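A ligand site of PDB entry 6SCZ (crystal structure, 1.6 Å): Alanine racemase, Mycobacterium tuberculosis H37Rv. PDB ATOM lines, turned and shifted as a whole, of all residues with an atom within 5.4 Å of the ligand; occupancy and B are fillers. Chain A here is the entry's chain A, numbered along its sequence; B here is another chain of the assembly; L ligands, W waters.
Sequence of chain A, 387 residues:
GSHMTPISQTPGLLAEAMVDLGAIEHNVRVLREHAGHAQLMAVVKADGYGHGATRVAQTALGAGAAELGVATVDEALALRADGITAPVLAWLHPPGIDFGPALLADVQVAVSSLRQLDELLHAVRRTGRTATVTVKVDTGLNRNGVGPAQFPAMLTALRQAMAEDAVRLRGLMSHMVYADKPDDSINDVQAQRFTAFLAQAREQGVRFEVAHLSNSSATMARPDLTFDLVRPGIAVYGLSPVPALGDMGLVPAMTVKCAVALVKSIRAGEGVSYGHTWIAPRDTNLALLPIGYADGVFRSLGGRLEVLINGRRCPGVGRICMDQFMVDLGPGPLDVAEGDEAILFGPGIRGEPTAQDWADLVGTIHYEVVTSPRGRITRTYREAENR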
ATOM      1  N   VAL A  43      15.074  21.213  10.122  1.00  0.00           N
ATOM      2  CA  VAL A  43      13.976  22.081  10.500  1.00  0.00           C
ATOM      3  C   VAL A  43      14.524  23.283  11.264  1.00  0.00           C
ATOM      4  O   VAL A  43      15.119  23.131  12.333  1.00  0.00           O
ATOM      5  CB  VAL A  43      12.929  21.315  11.323  1.00  0.00           C
ATOM      6  CG1 VAL A  43      11.823  22.243  11.761  1.00  0.00           C
ATOM      7  CG2 VAL A  43      12.347  20.163  10.460  1.00  0.00           C
ATOM      8  N   LYS A  45      12.627  26.314  11.708  1.00  0.00           N
ATOM      9  CA  LYS A  45      11.571  27.232  12.090  1.00  0.00           C
ATOM     10  C   LYS A  45      11.897  27.882  13.444  1.00  0.00           C
ATOM     11  O   LYS A  45      12.808  27.461  14.166  1.00  0.00           O
ATOM     12  CB  LYS A  45      10.227  26.504  12.150  1.00  0.00           C
ATOM     13  CG  LYS A  45      10.117  25.470  13.264  1.00  0.00           C
ATOM     14  CD  LYS A  45       8.812  24.667  13.150  1.00  0.00           C
ATOM     15  CE  LYS A  45       8.181  24.464  14.508  1.00  0.00           C
ATOM     16  NZ  LYS A  45       6.818  23.865  14.384  1.00  0.00           N
ATOM     17  N   TYR A  49      14.966  27.298  16.150  1.00  0.00           N
ATOM     18  CA  TYR A  49      14.705  26.975  17.552  1.00  0.00           C
ATOM     19  C   TYR A  49      15.526  27.883  18.457  1.00  0.00           C
ATOM     20  O   TYR A  49      16.114  27.446  19.448  1.00  0.00           O
ATOM     21  CB  TYR A  49      15.024  25.510  17.866  1.00  0.00           C
ATOM     22  CG  TYR A  49      14.107  24.439  17.289  1.00  0.00           C
ATOM     23  CD1 TYR A  49      13.343  24.668  16.150  1.00  0.00           C
ATOM     24  CD2 TYR A  49      14.048  23.186  17.881  1.00  0.00           C
ATOM     25  CE1 TYR A  49      12.557  23.677  15.630  1.00  0.00           C
ATOM     26  CE2 TYR A  49      13.246  22.184  17.367  1.00  0.00           C
ATOM     27  CZ  TYR A  49      12.489  22.442  16.233  1.00  0.00           C
ATOM     28  OH  TYR A  49      11.699  21.463  15.693  1.00  0.00           O
ATOM     29  N   TRP A  91       5.126  25.000   5.762  1.00  0.00           N
ATOM     30  CA  TRP A  91       3.949  24.174   5.948  1.00  0.00           C
ATOM     31  C   TRP A  91       2.845  24.737   6.838  1.00  0.00           C
ATOM     32  O   TRP A  91       1.871  24.015   7.077  1.00  0.00           O
ATOM     33  CB  TRP A  91       4.350  22.809   6.501  1.00  0.00           C
ATOM     34  CG  TRP A  91       5.185  22.860   7.709  1.00  0.00           C
ATOM     35  CD1 TRP A  91       4.823  23.296   8.938  1.00  0.00           C
ATOM     36  CD2 TRP A  91       6.548  22.437   7.819  1.00  0.00           C
ATOM     37  NE1 TRP A  91       5.874  23.179   9.821  1.00  0.00           N
ATOM     38  CE2 TRP A  91       6.953  22.658   9.155  1.00  0.00           C
ATOM     39  CE3 TRP A  91       7.474  21.901   6.918  1.00  0.00           C
ATOM     40  CZ2 TRP A  91       8.230  22.355   9.606  1.00  0.00           C
ATOM     41  CZ3 TRP A  91       8.751  21.598   7.369  1.00  0.00           C
ATOM     42  CH2 TRP A  91       9.113  21.827   8.708  1.00  0.00           C
ATOM     43  N   LYS A 136       0.568  17.845   2.974  1.00  0.00           N
ATOM     44  CA  LYS A 136       0.678  17.465   4.371  1.00  0.00           C
ATOM     45  C   LYS A 136      -0.597  16.743   4.767  1.00  0.00           C
ATOM     46  O   LYS A 136      -1.686  17.327   4.737  1.00  0.00           O
ATOM     47  CB  LYS A 136       0.897  18.702   5.244  1.00  0.00           C
ATOM     48  CG  LYS A 136       1.153  18.401   6.704  1.00  0.00           C
ATOM     49  CD  LYS A 136       1.755  19.635   7.396  1.00  0.00           C
ATOM     50  CE  LYS A 136       2.094  19.331   8.831  1.00  0.00           C
ATOM     51  NZ  LYS A 136       0.870  19.229   9.681  1.00  0.00           N
ATOM     52  N   ARG A 143      -4.204  17.793  13.847  1.00  0.00           N
ATOM     53  CA  ARG A 143      -4.047  19.242  13.890  1.00  0.00           C
ATOM     54  C   ARG A 143      -4.458  19.779  12.531  1.00  0.00           C
ATOM     55  O   ARG A 143      -5.653  19.875  12.251  1.00  0.00           O
ATOM     56  CB  ARG A 143      -2.621  19.636  14.276  1.00  0.00           C
ATOM     57  CG  ARG A 143      -2.355  19.446  15.765  1.00  0.00           C
ATOM     58  CD  ARG A 143      -1.310  20.389  16.304  1.00  0.00           C
ATOM     59  NE  ARG A 143      -0.062  20.317  15.535  1.00  0.00           N
ATOM     60  CZ  ARG A 143       1.126  20.031  16.054  1.00  0.00           C
ATOM     61  NH1 ARG A 143       2.191  20.009  15.265  1.00  0.00           N
ATOM     62  NH2 ARG A 143       1.284  19.768  17.353  1.00  0.00           N
ATOM     63  N   MET A 173       3.912  14.491   3.088  1.00  0.00           N
ATOM     64  CA  MET A 173       4.470  14.571   4.432  1.00  0.00           C
ATOM     65  C   MET A 173       3.385  14.371   5.468  1.00  0.00           C
ATOM     66  O   MET A 173       2.208  14.666   5.239  1.00  0.00           O
ATOM     67  CB  MET A 173       5.197  15.917   4.676  1.00  0.00           C
ATOM     68  CG  MET A 173       4.271  17.123   4.887  1.00  0.00           C
ATOM     69  SD  MET A 173       5.114  18.708   5.074  1.00  0.00           S
ATOM     70  CE  MET A 173       5.674  18.602   6.790  1.00  0.00           C
ATOM     71  N   HIS A 175       3.294  14.205  10.207  1.00  0.00           N
ATOM     72  CA  HIS A 175       4.047  14.467  11.421  1.00  0.00           C
ATOM     73  C   HIS A 175       3.566  13.537  12.524  1.00  0.00           C
ATOM     74  O   HIS A 175       2.367  13.225  12.629  1.00  0.00           O
ATOM     75  CB  HIS A 175       3.891  15.945  11.811  1.00  0.00           C
ATOM     76  CG  HIS A 175       4.885  16.426  12.816  1.00  0.00           C
ATOM     77  ND1 HIS A 175       6.221  16.114  12.756  1.00  0.00           N
ATOM     78  CD2 HIS A 175       4.720  17.189  13.924  1.00  0.00           C
ATOM     79  CE1 HIS A 175       6.853  16.666  13.783  1.00  0.00           C
ATOM     80  NE2 HIS A 175       5.954  17.324  14.507  1.00  0.00           N
ATOM     81  N   ALA A 179       6.762  13.130  19.829  1.00  0.00           N
ATOM     82  CA  ALA A 179       8.086  13.646  19.520  1.00  0.00           C
ATOM     83  C   ALA A 179       9.179  12.909  20.267  1.00  0.00           C
ATOM     84  O   ALA A 179      10.352  13.043  19.892  1.00  0.00           O
ATOM     85  CB  ALA A 179       8.163  15.142  19.847  1.00  0.00           C
ATOM     86  N   ASN A 215      10.414  12.765  12.376  1.00  0.00           N
ATOM     87  CA  ASN A 215      11.041  13.812  13.161  1.00  0.00           C
ATOM     88  C   ASN A 215      12.358  13.271  13.715  1.00  0.00           C
ATOM     89  O   ASN A 215      12.832  12.196  13.327  1.00  0.00           O
ATOM     90  CB  ASN A 215      10.091  14.272  14.265  1.00  0.00           C
ATOM     91  CG  ASN A 215       9.651  13.127  15.175  1.00  0.00           C
ATOM     92  OD1 ASN A 215      10.143  12.005  15.090  1.00  0.00           O
ATOM     93  ND2 ASN A 215       8.713  13.429  16.047  1.00  0.00           N
ATOM     94  N   SER A 216      12.965  13.997  14.660  1.00  0.00           N
ATOM     95  CA  SER A 216      14.243  13.573  15.227  1.00  0.00           C
ATOM     96  C   SER A 216      14.103  12.231  15.915  1.00  0.00           C
ATOM     97  O   SER A 216      14.962  11.358  15.779  1.00  0.00           O
ATOM     98  CB  SER A 216      14.733  14.611  16.244  1.00  0.00           C
ATOM     99  OG  SER A 216      15.122  15.830  15.648  1.00  0.00           O
ATOM    100  N   SER A 217      13.044  12.054  16.689  1.00  0.00           N
ATOM    101  CA  SER A 217      12.863  10.812  17.422  1.00  0.00           C
ATOM    102  C   SER A 217      12.836   9.627  16.475  1.00  0.00           C
ATOM    103  O   SER A 217      13.584   8.656  16.644  1.00  0.00           O
ATOM    104  CB  SER A 217      11.560  10.855  18.231  1.00  0.00           C
ATOM    105  OG  SER A 217      11.345   9.574  18.800  1.00  0.00           O
ATOM    106  N   ARG A 231      13.044  14.553   8.672  1.00  0.00           N
ATOM    107  CA  ARG A 231      12.725  15.952   8.920  1.00  0.00           C
ATOM    108  C   ARG A 231      13.026  16.308  10.371  1.00  0.00           C
ATOM    109  O   ARG A 231      12.140  16.693  11.126  1.00  0.00           O
ATOM    110  CB  ARG A 231      11.265  16.206   8.572  1.00  0.00           C
ATOM    111  CG  ARG A 231      10.928  17.609   8.163  1.00  0.00           C
ATOM    112  CD  ARG A 231       9.469  17.680   7.642  1.00  0.00           C
ATOM    113  NE  ARG A 231       8.526  17.191   8.649  1.00  0.00           N
ATOM    114  CZ  ARG A 231       7.824  16.056   8.599  1.00  0.00           C
ATOM    115  NH1 ARG A 231       7.852  15.258   7.537  1.00  0.00           N
ATOM    116  NH2 ARG A 231       7.058  15.740   9.652  1.00  0.00           N
ATOM    117  N   PRO A 232      14.291  16.192  10.799  1.00  0.00           N
ATOM    118  CA  PRO A 232      14.616  16.473  12.207  1.00  0.00           C
ATOM    119  C   PRO A 232      14.804  17.951  12.491  1.00  0.00           C
ATOM    120  O   PRO A 232      15.390  18.706  11.717  1.00  0.00           O
ATOM    121  CB  PRO A 232      15.925  15.702  12.407  1.00  0.00           C
ATOM    122  CG  PRO A 232      16.571  15.732  11.069  1.00  0.00           C
ATOM    123  CD  PRO A 232      15.444  15.643  10.071  1.00  0.00           C
ATOM    124  N   GLY A 233      14.315  18.358  13.667  1.00  0.00           N
ATOM    125  CA  GLY A 233      14.594  19.674  14.199  1.00  0.00           C
ATOM    126  C   GLY A 233      15.447  19.599  15.455  1.00  0.00           C
ATOM    127  O   GLY A 233      16.635  19.931  15.426  1.00  0.00           O
ATOM    128  N   ILE A 234      14.854  19.114  16.553  1.00  0.00           N
ATOM    129  CA  ILE A 234      15.469  19.248  17.874  1.00  0.00           C
ATOM    130  C   ILE A 234      16.877  18.633  17.914  1.00  0.00           C
ATOM    131  O   ILE A 234      17.783  19.185  18.540  1.00  0.00           O
ATOM    132  CB  ILE A 234      14.535  18.650  18.941  1.00  0.00           C
ATOM    133  CG1 ILE A 234      14.923  19.053  20.372  1.00  0.00           C
ATOM    134  CG2 ILE A 234      14.474  17.149  18.852  1.00  0.00           C
ATOM    135  CD1 ILE A 234      14.873  20.532  20.634  1.00  0.00           C
ATOM    136  N   ALA A 235      17.099  17.512  17.209  1.00  0.00           N
ATOM    137  CA  ALA A 235      18.403  16.865  17.252  1.00  0.00           C
ATOM    138  C   ALA A 235      19.462  17.657  16.476  1.00  0.00           C
ATOM    139  O   ALA A 235      20.658  17.525  16.758  1.00  0.00           O
ATOM    140  CB  ALA A 235      18.295  15.433  16.719  1.00  0.00           C
ATOM    141  N   TYR A 367      12.812  22.037  24.143  1.00  0.00           N
ATOM    142  CA  TYR A 367      12.370  22.874  23.029  1.00  0.00           C
ATOM    143  C   TYR A 367      12.028  24.280  23.504  1.00  0.00           C
ATOM    144  O   TYR A 367      12.383  25.265  22.855  1.00  0.00           O
ATOM    145  CB  TYR A 367      11.124  22.295  22.362  1.00  0.00           C
ATOM    146  CG  TYR A 367      11.185  20.947  21.654  1.00  0.00           C
ATOM    147  CD1 TYR A 367      11.240  19.756  22.363  1.00  0.00           C
ATOM    148  CD2 TYR A 367      11.070  20.874  20.278  1.00  0.00           C
ATOM    149  CE1 TYR A 367      11.226  18.532  21.719  1.00  0.00           C
ATOM    150  CE2 TYR A 367      11.060  19.654  19.622  1.00  0.00           C
ATOM    151  CZ  TYR A 367      11.134  18.498  20.343  1.00  0.00           C
ATOM    152  OH  TYR A 367      11.122  17.275  19.709  1.00  0.00           O
ATOM    153  N   TYR B 274       0.340  16.672  20.461  1.00  0.00           N
ATOM    154  CA  TYR B 274       1.351  15.684  20.825  1.00  0.00           C
ATOM    155  C   TYR B 274       0.923  14.853  22.018  1.00  0.00           C
ATOM    156  O   TYR B 274       0.367  15.358  22.996  1.00  0.00           O
ATOM    157  CB  TYR B 274       2.676  16.385  21.109  1.00  0.00           C
ATOM    158  CG  TYR B 274       3.245  17.106  19.913  1.00  0.00           C
ATOM    159  CD1 TYR B 274       3.423  16.436  18.709  1.00  0.00           C
ATOM    160  CD2 TYR B 274       3.557  18.451  19.970  1.00  0.00           C
ATOM    161  CE1 TYR B 274       3.929  17.093  17.601  1.00  0.00           C
ATOM    162  CE2 TYR B 274       4.058  19.116  18.863  1.00  0.00           C
ATOM    163  CZ  TYR B 274       4.245  18.426  17.679  1.00  0.00           C
ATOM    164  OH  TYR B 274       4.740  19.100  16.574  1.00  0.00           O
ATOM    165  N   TYR B 293       4.725  28.391  22.194  1.00  0.00           N
ATOM    166  CA  TYR B 293       5.600  28.795  23.285  1.00  0.00           C
ATOM    167  C   TYR B 293       6.831  29.548  22.795  1.00  0.00           C
ATOM    168  O   TYR B 293       7.394  30.337  23.570  1.00  0.00           O
ATOM    169  CB  TYR B 293       5.995  27.603  24.182  1.00  0.00           C
ATOM    170  CG  TYR B 293       6.580  26.395  23.499  1.00  0.00           C
ATOM    171  CD1 TYR B 293       7.859  26.421  22.996  1.00  0.00           C
ATOM    172  CD2 TYR B 293       5.856  25.205  23.387  1.00  0.00           C
ATOM    173  CE1 TYR B 293       8.423  25.322  22.394  1.00  0.00           C
ATOM    174  CE2 TYR B 293       6.415  24.082  22.757  1.00  0.00           C
ATOM    175  CZ  TYR B 293       7.709  24.165  22.266  1.00  0.00           C
ATOM    176  OH  TYR B 293       8.298  23.099  21.621  1.00  0.00           O
ATOM    177  N   CYS B 321       2.137  23.837  21.318  1.00  0.00           N
ATOM    178  CA  CYS B 321       3.291  23.492  20.498  1.00  0.00           C
ATOM    179  C   CYS B 321       4.187  24.715  20.376  1.00  0.00           C
ATOM    180  O   CYS B 321       3.896  25.786  20.906  1.00  0.00           O
ATOM    181  CB  CYS B 321       2.838  22.978  19.129  1.00  0.00           C
ATOM    182  SG  CYS B 321       1.690  21.621  19.279  1.00  0.00           S
ATOM    183  N   MET B 322       5.292  24.553  19.670  1.00  0.00           N
ATOM    184  CA  MET B 322       6.227  25.658  19.535  1.00  0.00           C
ATOM    185  C   MET B 322       5.577  26.870  18.882  1.00  0.00           C
ATOM    186  O   MET B 322       5.876  28.014  19.245  1.00  0.00           O
ATOM    187  CB  MET B 322       7.456  25.216  18.732  1.00  0.00           C
ATOM    188  CG  MET B 322       8.559  26.270  18.643  1.00  0.00           C
ATOM    189  SD  MET B 322      10.028  25.680  17.790  1.00  0.00           S
ATOM    190  CE  MET B 322      10.648  24.505  18.984  1.00  0.00           C
ATOM    191  N   ASP B 323       4.657  26.637  17.927  1.00  0.00           N
ATOM    192  CA  ASP B 323       4.125  27.718  17.103  1.00  0.00           C
ATOM    193  C   ASP B 323       2.615  27.642  16.925  1.00  0.00           C
ATOM    194  O   ASP B 323       2.079  28.340  16.052  1.00  0.00           O
ATOM    195  CB  ASP B 323       4.795  27.708  15.720  1.00  0.00           C
ATOM    196  CG  ASP B 323       4.303  26.557  14.829  1.00  0.00           C
ATOM    197  OD1 ASP B 323       3.746  25.573  15.351  1.00  0.00           O
ATOM    198  OD2 ASP B 323       4.475  26.622  13.594  1.00  0.00           O
ATOM    199  N   GLN B 324       1.908  26.852  17.719  1.00  0.00           N
ATOM    200  CA  GLN B 324       0.464  26.755  17.575  1.00  0.00           C
ATOM    201  C   GLN B 324      -0.121  26.047  18.785  1.00  0.00           C
ATOM    202  O   GLN B 324       0.579  25.319  19.494  1.00  0.00           O
ATOM    203  CB  GLN B 324       0.072  26.005  16.302  1.00  0.00           C
ATOM    204  CG  GLN B 324       0.553  24.574  16.323  1.00  0.00           C
ATOM    205  CD  GLN B 324       0.344  23.876  15.021  1.00  0.00           C
ATOM    206  OE1 GLN B 324      -0.675  23.213  14.806  1.00  0.00           O
ATOM    207  NE2 GLN B 324       1.314  24.020  14.119  1.00  0.00           N
HETATM  208  C1  LIG L   1       7.392  20.065  12.705  1.00  0.00           C
HETATM  209  C2  LIG L   1       8.514  19.827  13.482  1.00  0.00           C
HETATM  210  C3  LIG L   1       9.482  18.932  13.010  1.00  0.00           C
HETATM  211  C4  LIG L   1       9.298  18.303  11.768  1.00  0.00           C
HETATM  212  C5  LIG L   1       7.244  19.397  11.487  1.00  0.00           C
HETATM  213  N1  LIG L   1       7.541  20.069  15.695  1.00  0.00           N
HETATM  214  C6  LIG L   1       7.436  20.694  16.975  1.00  0.00           C
HETATM  215  C7  LIG L   1       6.285  21.451  17.484  1.00  0.00           C
HETATM  216  O1  LIG L   1       5.013  21.499  16.770  1.00  0.00           O
HETATM  217  C8  LIG L   1       8.384  20.959  17.929  1.00  0.00           C
HETATM  218  O2  LIG L   1       7.773  21.679  18.926  1.00  0.00           O
HETATM  219  N2  LIG L   1       6.513  21.994  18.679  1.00  0.00           N
HETATM  220  C9  LIG L   1       6.043  19.633  10.598  1.00  0.00           C
HETATM  221  C10 LIG L   1       8.652  20.534  14.816  1.00  0.00           C
HETATM  222  C11 LIG L   1      10.737  18.613  13.785  1.00  0.00           C
HETATM  223  N3  LIG L   1       8.203  18.553  11.055  1.00  0.00           N
HETATM  224  O3  LIG L   1       6.442  20.906  13.124  1.00  0.00           O
HETATM  225  O4  LIG L   1      12.623  16.738  15.364  1.00  0.00           O
HETATM  226  O5  LIG L   1      12.125  18.951  16.403  1.00  0.00           O
HETATM  227  O6  LIG L   1      10.830  16.888  17.124  1.00  0.00           O
HETATM  228  O7  LIG L   1      10.368  17.873  14.931  1.00  0.00           O
HETATM  229  P1  LIG L   1      11.559  17.608  16.015  1.00  0.00           P
HETATM  230  O   HOH W   1      11.604  14.274  17.683  1.00  0.00           O
HETATM  231  O   HOH W   2       8.064  17.184  16.955  1.00  0.00           O
HETATM  232  O   HOH W   3       6.519  21.039  21.220  1.00  0.00           O
HETATM  233  O   HOH W   4       3.629  21.073  13.066  1.00  0.00           O
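N of Met 322 of chain B is in hydrogen-bond range of N2 of the ligand, at 3.0 Å.
The side-chain amino group (NZ) of Lys 45 is in hydrogen-bond range of an oxygen (O3) of the ligand (3.2 Å).
N3 of the ligand sits at hydrogen-bond distance from NE of Arg 231 (2.8 Å).
A nitrogen (N1) of the ligand sits at hydrogen-bond distance from a ring nitrogen (NE2) of His 175 (3.4 Å).
N of Ile 234 lies within hydrogen-bond range of O5 of the ligand (2.7 Å).
An oxygen (O4) of the ligand sits at hydrogen-bond distance from the side-chain hydroxyl of Ser 216, at 2.7 Å.
OH of Tyr 49 is in hydrogen-bond range of O5 of the ligand (2.6 Å).
OH of Tyr 293 of chain B lies within hydrogen-bond range of O2 of the ligand, 3.1 Å away.
The side-chain hydroxyl of Tyr 367 is in hydrogen-bond range of an oxygen (O6) of the ligand.
An oxygen (O1) of the ligand lies within hydrogen-bond range of the side-chain hydroxyl (OH) of Tyr 274 of chain B (2.4 Å).
The backbone NH (N) of Gly 233 is in hydrogen-bond range of an oxygen (O4) of the ligand, at 2.9 Å.
The backbone NH of Ser 216 sits at hydrogen-bond distance from an oxygen (O4) of the ligand, at 2.9 Å.
NH2 of Arg 231 lies within hydrogen-bond range of ND1 of His 175, 3.2 Å away.
The backbone NH (N) of Tyr 293 of chain B sits at hydrogen-bond distance from the backbone carbonyl oxygen (O) of Met 322 of chain B, 3.2 Å away.
The side-chain hydroxyl (OG) of Ser 216 sits at hydrogen-bond distance from the backbone NH (N) of Ile 234, 3.4 Å away.
The side-chain amide oxygen (OD1) of Asn 215 sits close to the backbone NH (N) of Ser 217.
The guanidinium group (NE) of Arg 143 lies within hydrogen-bond range of the side-chain amide oxygen (OE1) of Gln 324 of chain B (3.0 Å).
N of Tyr 293 of chain B sits at hydrogen-bond distance from O of Cys 321 of chain B.
The backbone NH (N) of Ala 235 is in hydrogen-bond range of the side-chain hydroxyl (OG) of Ser 216, at 3.0 Å.
The guanidinium group of Arg 143 sits at hydrogen-bond distance from the side-chain hydroxyl of Tyr 274 of chain B (3.0 Å).
Merely in contact with the ligand: Trp 91, Arg 143, Cys 321 of chain B, Asn 215, Pro 232, Val 43 and Met 173.
Hydrophobic or aromatic side chains that line the ligand: Val 43, Tyr 49, Trp 91, Met 173, His 175, Ile 234, Tyr 367, Tyr 274 of chain B and Met 322 of chain B.
18 residues have an atom within 4 Å of the ligand: Val 43, Lys 45, Tyr 49, Trp 91, Arg 143, Met 173, His 175, Asn 215, Ser 216, Arg 231, Pro 232, Gly 233, Ile 234, Tyr 367, Tyr 274 of chain B, Tyr 293 of chain B, Cys 321 of chain B and Met 322 of chain B.
The nearest printed residue that does not touch the ligand is Ala 179 (4.2 Å).
Water W3 lies within hydrogen-bond range of an oxygen (O2) of the ligand and the side-chain hydroxyl (OH) of Tyr 293 of chain B.
Water W2 lies within hydrogen-bond range of O6 of the ligand and NE2 of His 175.
Water W4 bridges an oxygen (O3) of the ligand and the guanidinium group of Arg 143.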
